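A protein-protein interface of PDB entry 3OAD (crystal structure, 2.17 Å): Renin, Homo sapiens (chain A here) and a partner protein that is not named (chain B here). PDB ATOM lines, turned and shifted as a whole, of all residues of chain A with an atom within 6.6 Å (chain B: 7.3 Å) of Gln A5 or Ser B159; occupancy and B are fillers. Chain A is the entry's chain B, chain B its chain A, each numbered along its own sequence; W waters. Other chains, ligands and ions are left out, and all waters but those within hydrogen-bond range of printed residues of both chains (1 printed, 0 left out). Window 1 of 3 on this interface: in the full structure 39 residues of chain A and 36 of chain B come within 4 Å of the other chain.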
ATOM      1  N   LEU A   2       7.761  16.998 -20.427  1.00  0.00           N
ATOM      2  CA  LEU A   2       8.981  17.761 -20.187  1.00  0.00           C
ATOM      3  C   LEU A   2       9.645  17.262 -18.917  1.00  0.00           C
ATOM      4  O   LEU A   2       9.007  17.210 -17.881  1.00  0.00           O
ATOM      5  CB  LEU A   2       8.627  19.246 -20.014  1.00  0.00           C
ATOM      6  CG  LEU A   2       9.780  20.175 -19.628  1.00  0.00           C
ATOM      7  CD1 LEU A   2      10.813  20.128 -20.723  1.00  0.00           C
ATOM      8  CD2 LEU A   2       9.320  21.615 -19.376  1.00  0.00           C
ATOM      9  N   GLY A   3      10.922  16.915 -18.982  1.00  0.00           N
ATOM     10  CA  GLY A   3      11.625  16.336 -17.828  1.00  0.00           C
ATOM     11  C   GLY A   3      12.005  17.333 -16.736  1.00  0.00           C
ATOM     12  O   GLY A   3      12.240  16.945 -15.583  1.00  0.00           O
ATOM     13  N   GLY A   4      12.068  18.613 -17.113  1.00  0.00           N
ATOM     14  CA  GLY A   4      12.427  19.714 -16.220  1.00  0.00           C
ATOM     15  C   GLY A   4      12.934  20.909 -17.010  1.00  0.00           C
ATOM     16  O   GLY A   4      12.908  20.883 -18.237  1.00  0.00           O
ATOM     17  N   GLN A   5      13.435  21.932 -16.308  1.00  0.00           N
ATOM     18  CA  GLN A   5      13.876  23.187 -16.955  1.00  0.00           C
ATOM     19  C   GLN A   5      14.715  24.123 -16.084  1.00  0.00           C
ATOM     20  O   GLN A   5      14.376  24.391 -14.933  1.00  0.00           O
ATOM     21  CB  GLN A   5      12.664  23.961 -17.434  1.00  0.00           C
ATOM     22  CG  GLN A   5      13.010  25.312 -17.999  1.00  0.00           C
ATOM     23  CD  GLN A   5      11.800  26.185 -18.100  1.00  0.00           C
ATOM     24  OE1 GLN A   5      11.314  26.709 -17.095  1.00  0.00           O
ATOM     25  NE2 GLN A   5      11.284  26.335 -19.313  1.00  0.00           N
ATOM     26  N   ILE A   6      15.811  24.630 -16.639  1.00  0.00           N
ATOM     27  CA  ILE A   6      16.551  25.704 -15.980  1.00  0.00           C
ATOM     28  C   ILE A   6      16.302  27.013 -16.732  1.00  0.00           C
ATOM     29  O   ILE A   6      16.218  27.022 -17.957  1.00  0.00           O
ATOM     30  CB  ILE A   6      18.061  25.422 -15.871  1.00  0.00           C
ATOM     31  CG1 ILE A   6      18.772  26.580 -15.169  1.00  0.00           C
ATOM     32  CG2 ILE A   6      18.694  25.202 -17.252  1.00  0.00           C
ATOM     33  CD1 ILE A   6      20.255  26.300 -14.779  1.00  0.00           C
ATOM     34  N   VAL A   7      16.146  28.097 -15.973  1.00  0.00           N
ATOM     35  CA  VAL A   7      16.054  29.428 -16.529  1.00  0.00           C
ATOM     36  C   VAL A   7      17.240  30.242 -16.026  1.00  0.00           C
ATOM     37  O   VAL A   7      17.471  30.347 -14.830  1.00  0.00           O
ATOM     38  CB  VAL A   7      14.696  30.108 -16.196  1.00  0.00           C
ATOM     39  CG1 VAL A   7      14.577  31.473 -16.894  1.00  0.00           C
ATOM     40  CG2 VAL A   7      13.551  29.225 -16.644  1.00  0.00           C
ATOM     41  N   LEU A   8      18.033  30.753 -16.956  1.00  0.00           N
ATOM     42  CA  LEU A   8      19.056  31.719 -16.644  1.00  0.00           C
ATOM     43  C   LEU A   8      18.461  33.083 -16.887  1.00  0.00           C
ATOM     44  O   LEU A   8      17.980  33.369 -17.987  1.00  0.00           O
ATOM     45  CB  LEU A   8      20.276  31.530 -17.540  1.00  0.00           C
ATOM     46  CG  LEU A   8      20.825  30.111 -17.637  1.00  0.00           C
ATOM     47  CD1 LEU A   8      21.870  30.051 -18.751  1.00  0.00           C
ATOM     48  CD2 LEU A   8      21.399  29.651 -16.274  1.00  0.00           C
ATOM     49  N   GLY A   9      18.457  33.896 -15.839  1.00  0.00           N
ATOM     50  CA  GLY A   9      18.017  35.279 -15.932  1.00  0.00           C
ATOM     51  C   GLY A   9      16.689  35.530 -15.272  1.00  0.00           C
ATOM     52  O   GLY A   9      16.304  36.678 -15.077  1.00  0.00           O
ATOM     53  N   GLY A  10      15.986  34.458 -14.929  1.00  0.00           N
ATOM     54  CA  GLY A  10      14.660  34.567 -14.333  1.00  0.00           C
ATOM     55  C   GLY A  10      14.068  33.238 -13.930  1.00  0.00           C
ATOM     56  O   GLY A  10      14.787  32.273 -13.639  1.00  0.00           O
ATOM     57  N   SER A  11      12.746  33.188 -13.906  1.00  0.00           N
ATOM     58  CA  SER A  11      12.022  32.012 -13.476  1.00  0.00           C
ATOM     59  C   SER A  11      10.913  31.798 -14.443  1.00  0.00           C
ATOM     60  O   SER A  11      10.557  32.699 -15.193  1.00  0.00           O
ATOM     61  CB  SER A  11      11.425  32.212 -12.088  1.00  0.00           C
ATOM     62  OG  SER A  11      10.449  33.246 -12.099  1.00  0.00           O
ATOM     63  N   ASP A  12      10.342  30.605 -14.410  1.00  0.00           N
ATOM     64  CA  ASP A  12       9.206  30.357 -15.240  1.00  0.00           C
ATOM     65  C   ASP A  12       7.922  30.113 -14.421  1.00  0.00           C
ATOM     66  O   ASP A  12       7.771  29.063 -13.768  1.00  0.00           O
ATOM     67  CB  ASP A  12       9.517  29.256 -16.234  1.00  0.00           C
ATOM     68  CG  ASP A  12       8.444  29.090 -17.255  1.00  0.00           C
ATOM     69  OD1 ASP A  12       7.311  29.530 -17.027  1.00  0.00           O
ATOM     70  OD2 ASP A  12       8.716  28.478 -18.284  1.00  0.00           O
ATOM     71  N   GLN A  14       5.116  29.416 -15.382  1.00  0.00           N
ATOM     72  CA  GLN A  14       4.300  28.342 -15.928  1.00  0.00           C
ATOM     73  C   GLN A  14       4.511  27.053 -15.131  1.00  0.00           C
ATOM     74  O   GLN A  14       3.661  26.168 -15.151  1.00  0.00           O
ATOM     75  CB  GLN A  14       4.436  28.199 -17.471  1.00  0.00           C
ATOM     76  CG  GLN A  14       5.630  27.419 -18.051  1.00  0.00           C
ATOM     77  CD  GLN A  14       5.690  27.422 -19.622  1.00  0.00           C
ATOM     78  OE1 GLN A  14       6.754  27.692 -20.237  1.00  0.00           O
ATOM     79  NE2 GLN A  14       4.553  27.105 -20.261  1.00  0.00           N
ATOM     80  N   HIS A  15       5.601  27.004 -14.366  1.00  0.00           N
ATOM     81  CA  HIS A  15       5.993  25.786 -13.650  1.00  0.00           C
ATOM     82  C   HIS A  15       6.039  25.884 -12.121  1.00  0.00           C
ATOM     83  O   HIS A  15       6.506  24.963 -11.458  1.00  0.00           O
ATOM     84  CB  HIS A  15       7.310  25.257 -14.206  1.00  0.00           C
ATOM     85  CG  HIS A  15       7.191  24.710 -15.592  1.00  0.00           C
ATOM     86  ND1 HIS A  15       8.000  25.122 -16.627  1.00  0.00           N
ATOM     87  CD2 HIS A  15       6.342  23.799 -16.118  1.00  0.00           C
ATOM     88  CE1 HIS A  15       7.663  24.480 -17.729  1.00  0.00           C
ATOM     89  NE2 HIS A  15       6.656  23.674 -17.446  1.00  0.00           N
ATOM     90  N   TYR A  16       5.543  26.999 -11.574  1.00  0.00           N
ATOM     91  CA  TYR A  16       5.308  27.122 -10.130  1.00  0.00           C
ATOM     92  C   TYR A  16       4.025  27.887  -9.778  1.00  0.00           C
ATOM     93  O   TYR A  16       3.359  28.504 -10.650  1.00  0.00           O
ATOM     94  CB  TYR A  16       6.503  27.756  -9.421  1.00  0.00           C
ATOM     95  CG  TYR A  16       6.819  29.193  -9.798  1.00  0.00           C
ATOM     96  CD1 TYR A  16       7.798  29.482 -10.742  1.00  0.00           C
ATOM     97  CD2 TYR A  16       6.173  30.257  -9.170  1.00  0.00           C
ATOM     98  CE1 TYR A  16       8.107  30.802 -11.082  1.00  0.00           C
ATOM     99  CE2 TYR A  16       6.469  31.581  -9.492  1.00  0.00           C
ATOM    100  CZ  TYR A  16       7.431  31.852 -10.458  1.00  0.00           C
ATOM    101  OH  TYR A  16       7.739  33.168 -10.779  1.00  0.00           O
ATOM    102  N   PHE A  20       7.281  33.195  -4.555  1.00  0.00           N
ATOM    103  CA  PHE A  20       8.506  32.760  -3.937  1.00  0.00           C
ATOM    104  C   PHE A  20       8.549  33.203  -2.494  1.00  0.00           C
ATOM    105  O   PHE A  20       8.208  34.350  -2.189  1.00  0.00           O
ATOM    106  CB  PHE A  20       9.700  33.358  -4.683  1.00  0.00           C
ATOM    107  CG  PHE A  20      10.064  32.613  -5.934  1.00  0.00           C
ATOM    108  CD1 PHE A  20      10.511  31.285  -5.866  1.00  0.00           C
ATOM    109  CD2 PHE A  20       9.968  33.221  -7.172  1.00  0.00           C
ATOM    110  CE1 PHE A  20      10.851  30.587  -7.007  1.00  0.00           C
ATOM    111  CE2 PHE A  20      10.312  32.525  -8.319  1.00  0.00           C
ATOM    112  CZ  PHE A  20      10.756  31.195  -8.231  1.00  0.00           C
ATOM    113  N   TYR A 154       9.846  24.224  -6.795  1.00  0.00           N
ATOM    114  CA  TYR A 154      10.482  25.084  -7.803  1.00  0.00           C
ATOM    115  C   TYR A 154      11.454  26.045  -7.126  1.00  0.00           C
ATOM    116  O   TYR A 154      11.126  26.612  -6.096  1.00  0.00           O
ATOM    117  CB  TYR A 154       9.424  25.888  -8.562  1.00  0.00           C
ATOM    118  CG  TYR A 154      10.012  26.653  -9.743  1.00  0.00           C
ATOM    119  CD1 TYR A 154      10.678  27.884  -9.561  1.00  0.00           C
ATOM    120  CD2 TYR A 154       9.931  26.131 -11.029  1.00  0.00           C
ATOM    121  CE1 TYR A 154      11.233  28.571 -10.645  1.00  0.00           C
ATOM    122  CE2 TYR A 154      10.491  26.784 -12.100  1.00  0.00           C
ATOM    123  CZ  TYR A 154      11.132  28.005 -11.910  1.00  0.00           C
ATOM    124  OH  TYR A 154      11.669  28.624 -13.009  1.00  0.00           O
ATOM    125  N   THR A 155      12.656  26.216  -7.677  1.00  0.00           N
ATOM    126  CA  THR A 155      13.712  26.889  -6.902  1.00  0.00           C
ATOM    127  C   THR A 155      14.500  27.941  -7.652  1.00  0.00           C
ATOM    128  O   THR A 155      14.991  27.688  -8.763  1.00  0.00           O
ATOM    129  CB  THR A 155      14.703  25.884  -6.297  1.00  0.00           C
ATOM    130  OG1 THR A 155      13.969  24.973  -5.485  1.00  0.00           O
ATOM    131  CG2 THR A 155      15.735  26.586  -5.450  1.00  0.00           C
ATOM    132  N   GLU A 156      14.644  29.105  -7.010  1.00  0.00           N
ATOM    133  CA  GLU A 156      15.382  30.213  -7.594  1.00  0.00           C
ATOM    134  C   GLU A 156      16.642  30.451  -6.820  1.00  0.00           C
ATOM    135  O   GLU A 156      16.620  30.585  -5.590  1.00  0.00           O
ATOM    136  CB  GLU A 156      14.550  31.487  -7.632  1.00  0.00           C
ATOM    137  CG  GLU A 156      15.155  32.553  -8.520  1.00  0.00           C
ATOM    138  CD  GLU A 156      14.333  33.818  -8.549  1.00  0.00           C
ATOM    139  OE1 GLU A 156      14.416  34.612  -7.584  1.00  0.00           O
ATOM    140  OE2 GLU A 156      13.611  34.021  -9.548  1.00  0.00           O
ATOM    141  N   PHE A 157      17.757  30.496  -7.542  1.00  0.00           N
ATOM    142  CA  PHE A 157      19.029  30.777  -6.907  1.00  0.00           C
ATOM    143  C   PHE A 157      19.407  32.180  -7.326  1.00  0.00           C
ATOM    144  O   PHE A 157      19.637  32.438  -8.516  1.00  0.00           O
ATOM    145  CB  PHE A 157      20.077  29.765  -7.335  1.00  0.00           C
ATOM    146  CG  PHE A 157      19.733  28.359  -6.974  1.00  0.00           C
ATOM    147  CD1 PHE A 157      20.194  27.810  -5.768  1.00  0.00           C
ATOM    148  CD2 PHE A 157      18.939  27.592  -7.812  1.00  0.00           C
ATOM    149  CE1 PHE A 157      19.894  26.533  -5.405  1.00  0.00           C
ATOM    150  CE2 PHE A 157      18.607  26.306  -7.461  1.00  0.00           C
ATOM    151  CZ  PHE A 157      19.092  25.759  -6.244  1.00  0.00           C
ATOM    152  N   SER B   8      17.389  32.882 -20.580  1.00  0.00           N
ATOM    153  CA  SER B   8      17.647  31.697 -21.401  1.00  0.00           C
ATOM    154  C   SER B   8      17.240  30.434 -20.656  1.00  0.00           C
ATOM    155  O   SER B   8      17.651  30.207 -19.514  1.00  0.00           O
ATOM    156  CB  SER B   8      19.123  31.627 -21.814  1.00  0.00           C
ATOM    157  OG  SER B   8      19.448  30.394 -22.440  1.00  0.00           O
ATOM    158  N   SER B   9      16.415  29.622 -21.301  1.00  0.00           N
ATOM    159  CA  SER B   9      15.993  28.350 -20.726  1.00  0.00           C
ATOM    160  C   SER B   9      16.724  27.191 -21.404  1.00  0.00           C
ATOM    161  O   SER B   9      17.371  27.362 -22.434  1.00  0.00           O
ATOM    162  CB  SER B   9      14.493  28.182 -20.857  1.00  0.00           C
ATOM    163  OG  SER B   9      14.187  27.596 -22.108  1.00  0.00           O
ATOM    164  N   VAL B  10      16.623  26.017 -20.801  1.00  0.00           N
ATOM    165  CA  VAL B  10      17.306  24.818 -21.253  1.00  0.00           C
ATOM    166  C   VAL B  10      16.392  23.691 -20.800  1.00  0.00           C
ATOM    167  O   VAL B  10      16.190  23.490 -19.609  1.00  0.00           O
ATOM    168  CB  VAL B  10      18.712  24.683 -20.583  1.00  0.00           C
ATOM    169  CG1 VAL B  10      19.477  23.436 -21.056  1.00  0.00           C
ATOM    170  CG2 VAL B  10      19.559  25.943 -20.818  1.00  0.00           C
ATOM    171  N   ILE B  11      15.778  23.011 -21.752  1.00  0.00           N
ATOM    172  CA  ILE B  11      14.935  21.859 -21.458  1.00  0.00           C
ATOM    173  C   ILE B  11      15.830  20.776 -20.878  1.00  0.00           C
ATOM    174  O   ILE B  11      16.915  20.547 -21.403  1.00  0.00           O
ATOM    175  CB  ILE B  11      14.294  21.292 -22.753  1.00  0.00           C
ATOM    176  CG1 ILE B  11      13.450  22.354 -23.465  1.00  0.00           C
ATOM    177  CG2 ILE B  11      13.511  20.037 -22.468  1.00  0.00           C
ATOM    178  CD1 ILE B  11      12.388  23.028 -22.591  1.00  0.00           C
ATOM    179  N   LEU B  12      15.360  20.111 -19.820  1.00  0.00           N
ATOM    180  CA  LEU B  12      16.077  19.007 -19.203  1.00  0.00           C
ATOM    181  C   LEU B  12      15.409  17.682 -19.418  1.00  0.00           C
ATOM    182  O   LEU B  12      14.204  17.620 -19.653  1.00  0.00           O
ATOM    183  CB  LEU B  12      16.159  19.214 -17.698  1.00  0.00           C
ATOM    184  CG  LEU B  12      16.781  20.458 -17.087  1.00  0.00           C
ATOM    185  CD1 LEU B  12      16.854  20.202 -15.579  1.00  0.00           C
ATOM    186  CD2 LEU B  12      18.120  20.643 -17.669  1.00  0.00           C
ATOM    187  N   THR B  13      16.206  16.615 -19.295  1.00  0.00           N
ATOM    188  CA  THR B  13      15.724  15.231 -19.312  1.00  0.00           C
ATOM    189  C   THR B  13      15.672  14.690 -17.883  1.00  0.00           C
ATOM    190  O   THR B  13      16.645  14.819 -17.104  1.00  0.00           O
ATOM    191  CB  THR B  13      16.637  14.357 -20.177  1.00  0.00           C
ATOM    192  OG1 THR B  13      16.484  14.749 -21.529  1.00  0.00           O
ATOM    193  CG2 THR B  13      16.312  12.840 -20.093  1.00  0.00           C
ATOM    194  N   TYR B  20      18.969  14.447 -13.627  1.00  0.00           N
ATOM    195  CA  TYR B  20      18.366  15.537 -14.395  1.00  0.00           C
ATOM    196  C   TYR B  20      19.475  16.285 -15.108  1.00  0.00           C
ATOM    197  O   TYR B  20      20.413  16.830 -14.486  1.00  0.00           O
ATOM    198  CB  TYR B  20      17.609  16.467 -13.468  1.00  0.00           C
ATOM    199  CG  TYR B  20      16.333  15.897 -12.914  1.00  0.00           C
ATOM    200  CD1 TYR B  20      15.089  16.206 -13.501  1.00  0.00           C
ATOM    201  CD2 TYR B  20      16.346  15.098 -11.779  1.00  0.00           C
ATOM    202  CE1 TYR B  20      13.917  15.695 -12.959  1.00  0.00           C
ATOM    203  CE2 TYR B  20      15.201  14.592 -11.241  1.00  0.00           C
ATOM    204  CZ  TYR B  20      13.987  14.887 -11.823  1.00  0.00           C
ATOM    205  OH  TYR B  20      12.838  14.378 -11.280  1.00  0.00           O
ATOM    206  N   MET B 130      27.037  25.285 -10.761  1.00  0.00           N
ATOM    207  CA  MET B 130      26.364  26.553 -10.698  1.00  0.00           C
ATOM    208  C   MET B 130      26.597  27.206  -9.355  1.00  0.00           C
ATOM    209  O   MET B 130      25.852  28.114  -8.979  1.00  0.00           O
ATOM    210  CB  MET B 130      24.869  26.366 -10.900  1.00  0.00           C
ATOM    211  CG  MET B 130      24.494  25.709 -12.204  1.00  0.00           C
ATOM    212  SD  MET B 130      24.770  26.835 -13.564  1.00  0.00           S
ATOM    213  CE  MET B 130      23.439  28.017 -13.324  1.00  0.00           C
ATOM    214  N   PHE B 144      28.371  30.786 -14.482  1.00  0.00           N
ATOM    215  CA  PHE B 144      27.407  31.850 -14.192  1.00  0.00           C
ATOM    216  C   PHE B 144      28.074  33.142 -13.756  1.00  0.00           C
ATOM    217  O   PHE B 144      27.517  34.216 -13.931  1.00  0.00           O
ATOM    218  CB  PHE B 144      26.355  31.400 -13.177  1.00  0.00           C
ATOM    219  CG  PHE B 144      25.063  32.156 -13.281  1.00  0.00           C
ATOM    220  CD1 PHE B 144      24.271  32.054 -14.435  1.00  0.00           C
ATOM    221  CD2 PHE B 144      24.636  32.982 -12.241  1.00  0.00           C
ATOM    222  CE1 PHE B 144      23.044  32.755 -14.544  1.00  0.00           C
ATOM    223  CE2 PHE B 144      23.421  33.710 -12.341  1.00  0.00           C
ATOM    224  CZ  PHE B 144      22.617  33.587 -13.495  1.00  0.00           C
ATOM    225  N   VAL B 157      19.915  35.792 -11.476  1.00  0.00           N
ATOM    226  CA  VAL B 157      19.287  34.632 -10.870  1.00  0.00           C
ATOM    227  C   VAL B 157      19.187  33.509 -11.900  1.00  0.00           C
ATOM    228  O   VAL B 157      19.286  33.733 -13.104  1.00  0.00           O
ATOM    229  CB  VAL B 157      17.866  34.939 -10.294  1.00  0.00           C
ATOM    230  CG1 VAL B 157      17.863  36.210  -9.429  1.00  0.00           C
ATOM    231  CG2 VAL B 157      16.816  35.028 -11.402  1.00  0.00           C
ATOM    232  N   PHE B 158      19.047  32.291 -11.411  1.00  0.00           N
ATOM    233  CA  PHE B 158      18.710  31.153 -12.254  1.00  0.00           C
ATOM    234  C   PHE B 158      17.795  30.268 -11.430  1.00  0.00           C
ATOM    235  O   PHE B 158      17.945  30.195 -10.207  1.00  0.00           O
ATOM    236  CB  PHE B 158      19.950  30.418 -12.750  1.00  0.00           C
ATOM    237  CG  PHE B 158      20.850  29.933 -11.662  1.00  0.00           C
ATOM    238  CD1 PHE B 158      20.643  28.681 -11.074  1.00  0.00           C
ATOM    239  CD2 PHE B 158      21.917  30.710 -11.232  1.00  0.00           C
ATOM    240  CE1 PHE B 158      21.480  28.223 -10.093  1.00  0.00           C
ATOM    241  CE2 PHE B 158      22.769  30.263 -10.224  1.00  0.00           C
ATOM    242  CZ  PHE B 158      22.550  29.020  -9.653  1.00  0.00           C
ATOM    243  N   SER B 159      16.839  29.637 -12.110  1.00  0.00           N
ATOM    244  CA  SER B 159      15.771  28.859 -11.491  1.00  0.00           C
ATOM    245  C   SER B 159      15.748  27.422 -12.002  1.00  0.00           C
ATOM    246  O   SER B 159      16.098  27.164 -13.140  1.00  0.00           O
ATOM    247  CB  SER B 159      14.415  29.506 -11.799  1.00  0.00           C
ATOM    248  OG  SER B 159      14.465  30.910 -11.581  1.00  0.00           O
ATOM    249  N   PHE B 160      15.299  26.492 -11.164  1.00  0.00           N
ATOM    250  CA  PHE B 160      15.187  25.084 -11.574  1.00  0.00           C
ATOM    251  C   PHE B 160      13.751  24.588 -11.512  1.00  0.00           C
ATOM    252  O   PHE B 160      13.087  24.768 -10.510  1.00  0.00           O
ATOM    253  CB  PHE B 160      16.039  24.185 -10.665  1.00  0.00           C
ATOM    254  CG  PHE B 160      17.522  24.172 -10.983  1.00  0.00           C
ATOM    255  CD1 PHE B 160      18.328  25.248 -10.652  1.00  0.00           C
ATOM    256  CD2 PHE B 160      18.109  23.054 -11.559  1.00  0.00           C
ATOM    257  CE1 PHE B 160      19.711  25.240 -10.913  1.00  0.00           C
ATOM    258  CE2 PHE B 160      19.479  23.016 -11.821  1.00  0.00           C
ATOM    259  CZ  PHE B 160      20.285  24.122 -11.504  1.00  0.00           C
ATOM    260  N   TYR B 161      13.281  23.945 -12.569  1.00  0.00           N
ATOM    261  CA  TYR B 161      12.103  23.119 -12.456  1.00  0.00           C
ATOM    262  C   TYR B 161      12.518  21.663 -12.677  1.00  0.00           C
ATOM    263  O   TYR B 161      13.222  21.355 -13.625  1.00  0.00           O
ATOM    264  CB  TYR B 161      11.059  23.530 -13.473  1.00  0.00           C
ATOM    265  CG  TYR B 161       9.936  22.542 -13.682  1.00  0.00           C
ATOM    266  CD1 TYR B 161       9.043  22.250 -12.660  1.00  0.00           C
ATOM    267  CD2 TYR B 161       9.754  21.919 -14.913  1.00  0.00           C
ATOM    268  CE1 TYR B 161       8.015  21.340 -12.856  1.00  0.00           C
ATOM    269  CE2 TYR B 161       8.724  21.015 -15.119  1.00  0.00           C
ATOM    270  CZ  TYR B 161       7.861  20.739 -14.095  1.00  0.00           C
ATOM    271  OH  TYR B 161       6.821  19.855 -14.295  1.00  0.00           O
ATOM    272  N   TYR B 162      12.079  20.776 -11.799  1.00  0.00           N
ATOM    273  CA  TYR B 162      12.253  19.315 -11.995  1.00  0.00           C
ATOM    274  C   TYR B 162      10.866  18.639 -12.029  1.00  0.00           C
ATOM    275  O   TYR B 162      10.175  18.600 -11.009  1.00  0.00           O
ATOM    276  CB  TYR B 162      13.097  18.710 -10.862  1.00  0.00           C
ATOM    277  CG  TYR B 162      14.602  18.885 -10.940  1.00  0.00           C
ATOM    278  CD1 TYR B 162      15.210  19.464 -12.055  1.00  0.00           C
ATOM    279  CD2 TYR B 162      15.430  18.440  -9.893  1.00  0.00           C
ATOM    280  CE1 TYR B 162      16.606  19.618 -12.130  1.00  0.00           C
ATOM    281  CE2 TYR B 162      16.826  18.597  -9.942  1.00  0.00           C
ATOM    282  CZ  TYR B 162      17.409  19.193 -11.076  1.00  0.00           C
ATOM    283  OH  TYR B 162      18.772  19.357 -11.180  1.00  0.00           O
ATOM    284  N   ASN B 163      10.446  18.152 -13.201  1.00  0.00           N
ATOM    285  CA  ASN B 163       9.212  17.348 -13.354  1.00  0.00           C
ATOM    286  C   ASN B 163       9.318  15.992 -12.627  1.00  0.00           C
ATOM    287  O   ASN B 163      10.389  15.615 -12.146  1.00  0.00           O
ATOM    288  CB  ASN B 163       8.947  17.103 -14.835  1.00  0.00           C
ATOM    289  CG  ASN B 163       7.461  16.851 -15.157  1.00  0.00           C
ATOM    290  OD1 ASN B 163       6.622  16.701 -14.257  1.00  0.00           O
ATOM    291  ND2 ASN B 163       7.139  16.785 -16.453  1.00  0.00           N
HETATM  292  O   HOH W   1      11.962  16.940 -21.467  1.00  0.00           O
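Water W1 lies within hydrogen-bond range of the backbone NH of Gly A3 (2.7 Å) and the backbone carbonyl oxygen of Leu B12 (3.0 Å).
The side-chain amide oxygen (OE1) of Gln A5 sits close to the side-chain carboxylate (OD2) of Asp A12. The side-chain hydroxyl (OH) of Tyr B161 lies within hydrogen-bond range of the side-chain amide oxygen (OD1) of Asn B163 (3.2 Å). OG of Ser A11 sits at hydrogen-bond distance from OH of Tyr A16 (3.0 Å). OH of Tyr B20 sits at hydrogen-bond distance from O of Asn B163 (2.9 Å). N of Asp A12 is in hydrogen-bond range of OH of Tyr A154, 2.8 Å away.
OG of Ser B159 sits at hydrogen-bond distance from O of Gly A10 (2.5 Å). N of Phe B160 is in hydrogen-bond range of O of Thr A155 (2.7 Å). The backbone NH (N) of Ser B159 is in hydrogen-bond range of the backbone carbonyl oxygen (O) of Val A7 (2.9 Å). N of Tyr B161 lies within hydrogen-bond range of O of Gln A5 (2.6 Å). O of Leu A2 sits close to ND2 of Asn B163, 2.4 Å away. The backbone NH (N) of Val B10 sits at hydrogen-bond distance from the backbone carbonyl oxygen (O) of Ile A6 (3.0 Å). N of Asn B163 lies within hydrogen-bond range of O of Gly A3 (3.2 Å). N of Gly A9 lies within hydrogen-bond range of O of Val B157 (2.9 Å). N of Leu A8 sits at hydrogen-bond distance from O of Ser B8 (2.6 Å). The backbone carbonyl oxygen (O) of Gly A4 lies within hydrogen-bond range of the backbone NH (N) of Leu B12. The backbone carbonyl oxygen of Leu B12 sits close to the backbone NH of Gly A3. The backbone carbonyl oxygen (O) of Phe B158 sits at hydrogen-bond distance from the backbone NH (N) of Phe A157 (2.7 Å).
Of the 16 printed residues of chain B, 14 touch a printed residue of chain A. Of the 19 printed residues of chain A, 15 touch a printed residue of chain B.
Of the printed residues of chain B, Leu A2 touches Ile B11 (3.2 Å) and Asn B163 (2.4 Å). Printed residues of chain B within 4 Å of Gln A5: Val B10 (3.5 Å), Leu B12 (3.7 Å), Ser B159 (3.7 Å), Phe B160 (3.5 Å) and Tyr B161 (2.6 Å). Asp A12 touches none of the printed residues of chain B. Printed residues of chain A within 4 Å of Leu B12: Gly A3 (3.4 Å), Gly A4 (3.0 Å) and Gln A5 (3.7 Å). Printed residues of chain A within 4 Å of Tyr B20: Gly A3 (3.4 Å). Printed residues of chain A within 4 Å of Phe B158: Val A7 (3.0 Å), Leu A8 (3.9 Å), Glu A156 (3.6 Å) and Phe A157 (2.7 Å). Of chain A, only Gln A5 (3.7 Å), Ile A6 (3.2 Å), Val A7 (2.9 Å), Gly A10 (2.5 Å), Ser A11 (3.3 Å), Tyr A154 (3.1 Å), Thr A155 (3.1 Å) and Glu A156 (3.5 Å) come within 4 Å of Ser B159. Tyr B162 touches none of the printed residues of chain A. The nearest printed residue of chain B that does not touch Gln A5 is Ser B9 (4.01 Å).
Gly A3 touches Tyr B20 (O to CE1, 3.4 Å). Gly A4 touches Tyr B161 (CA to O, 3.2 Å). N of Gln A5 touches CG of Leu B12 (3.7 Å). C of Phe B160 touches O of Gln A5, 3.5 Å away. O of Ile A6 touches O of Ser B8, at 3.8 Å. Val A7 touches Ser B8 (CA to O, 3.5 Å). Met B130 touches Leu A8. Phe B158 touches Leu A8. CA of Ser B159 touches O of Thr A155, at 3.1 Å. Phe A157 touches Val B157.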
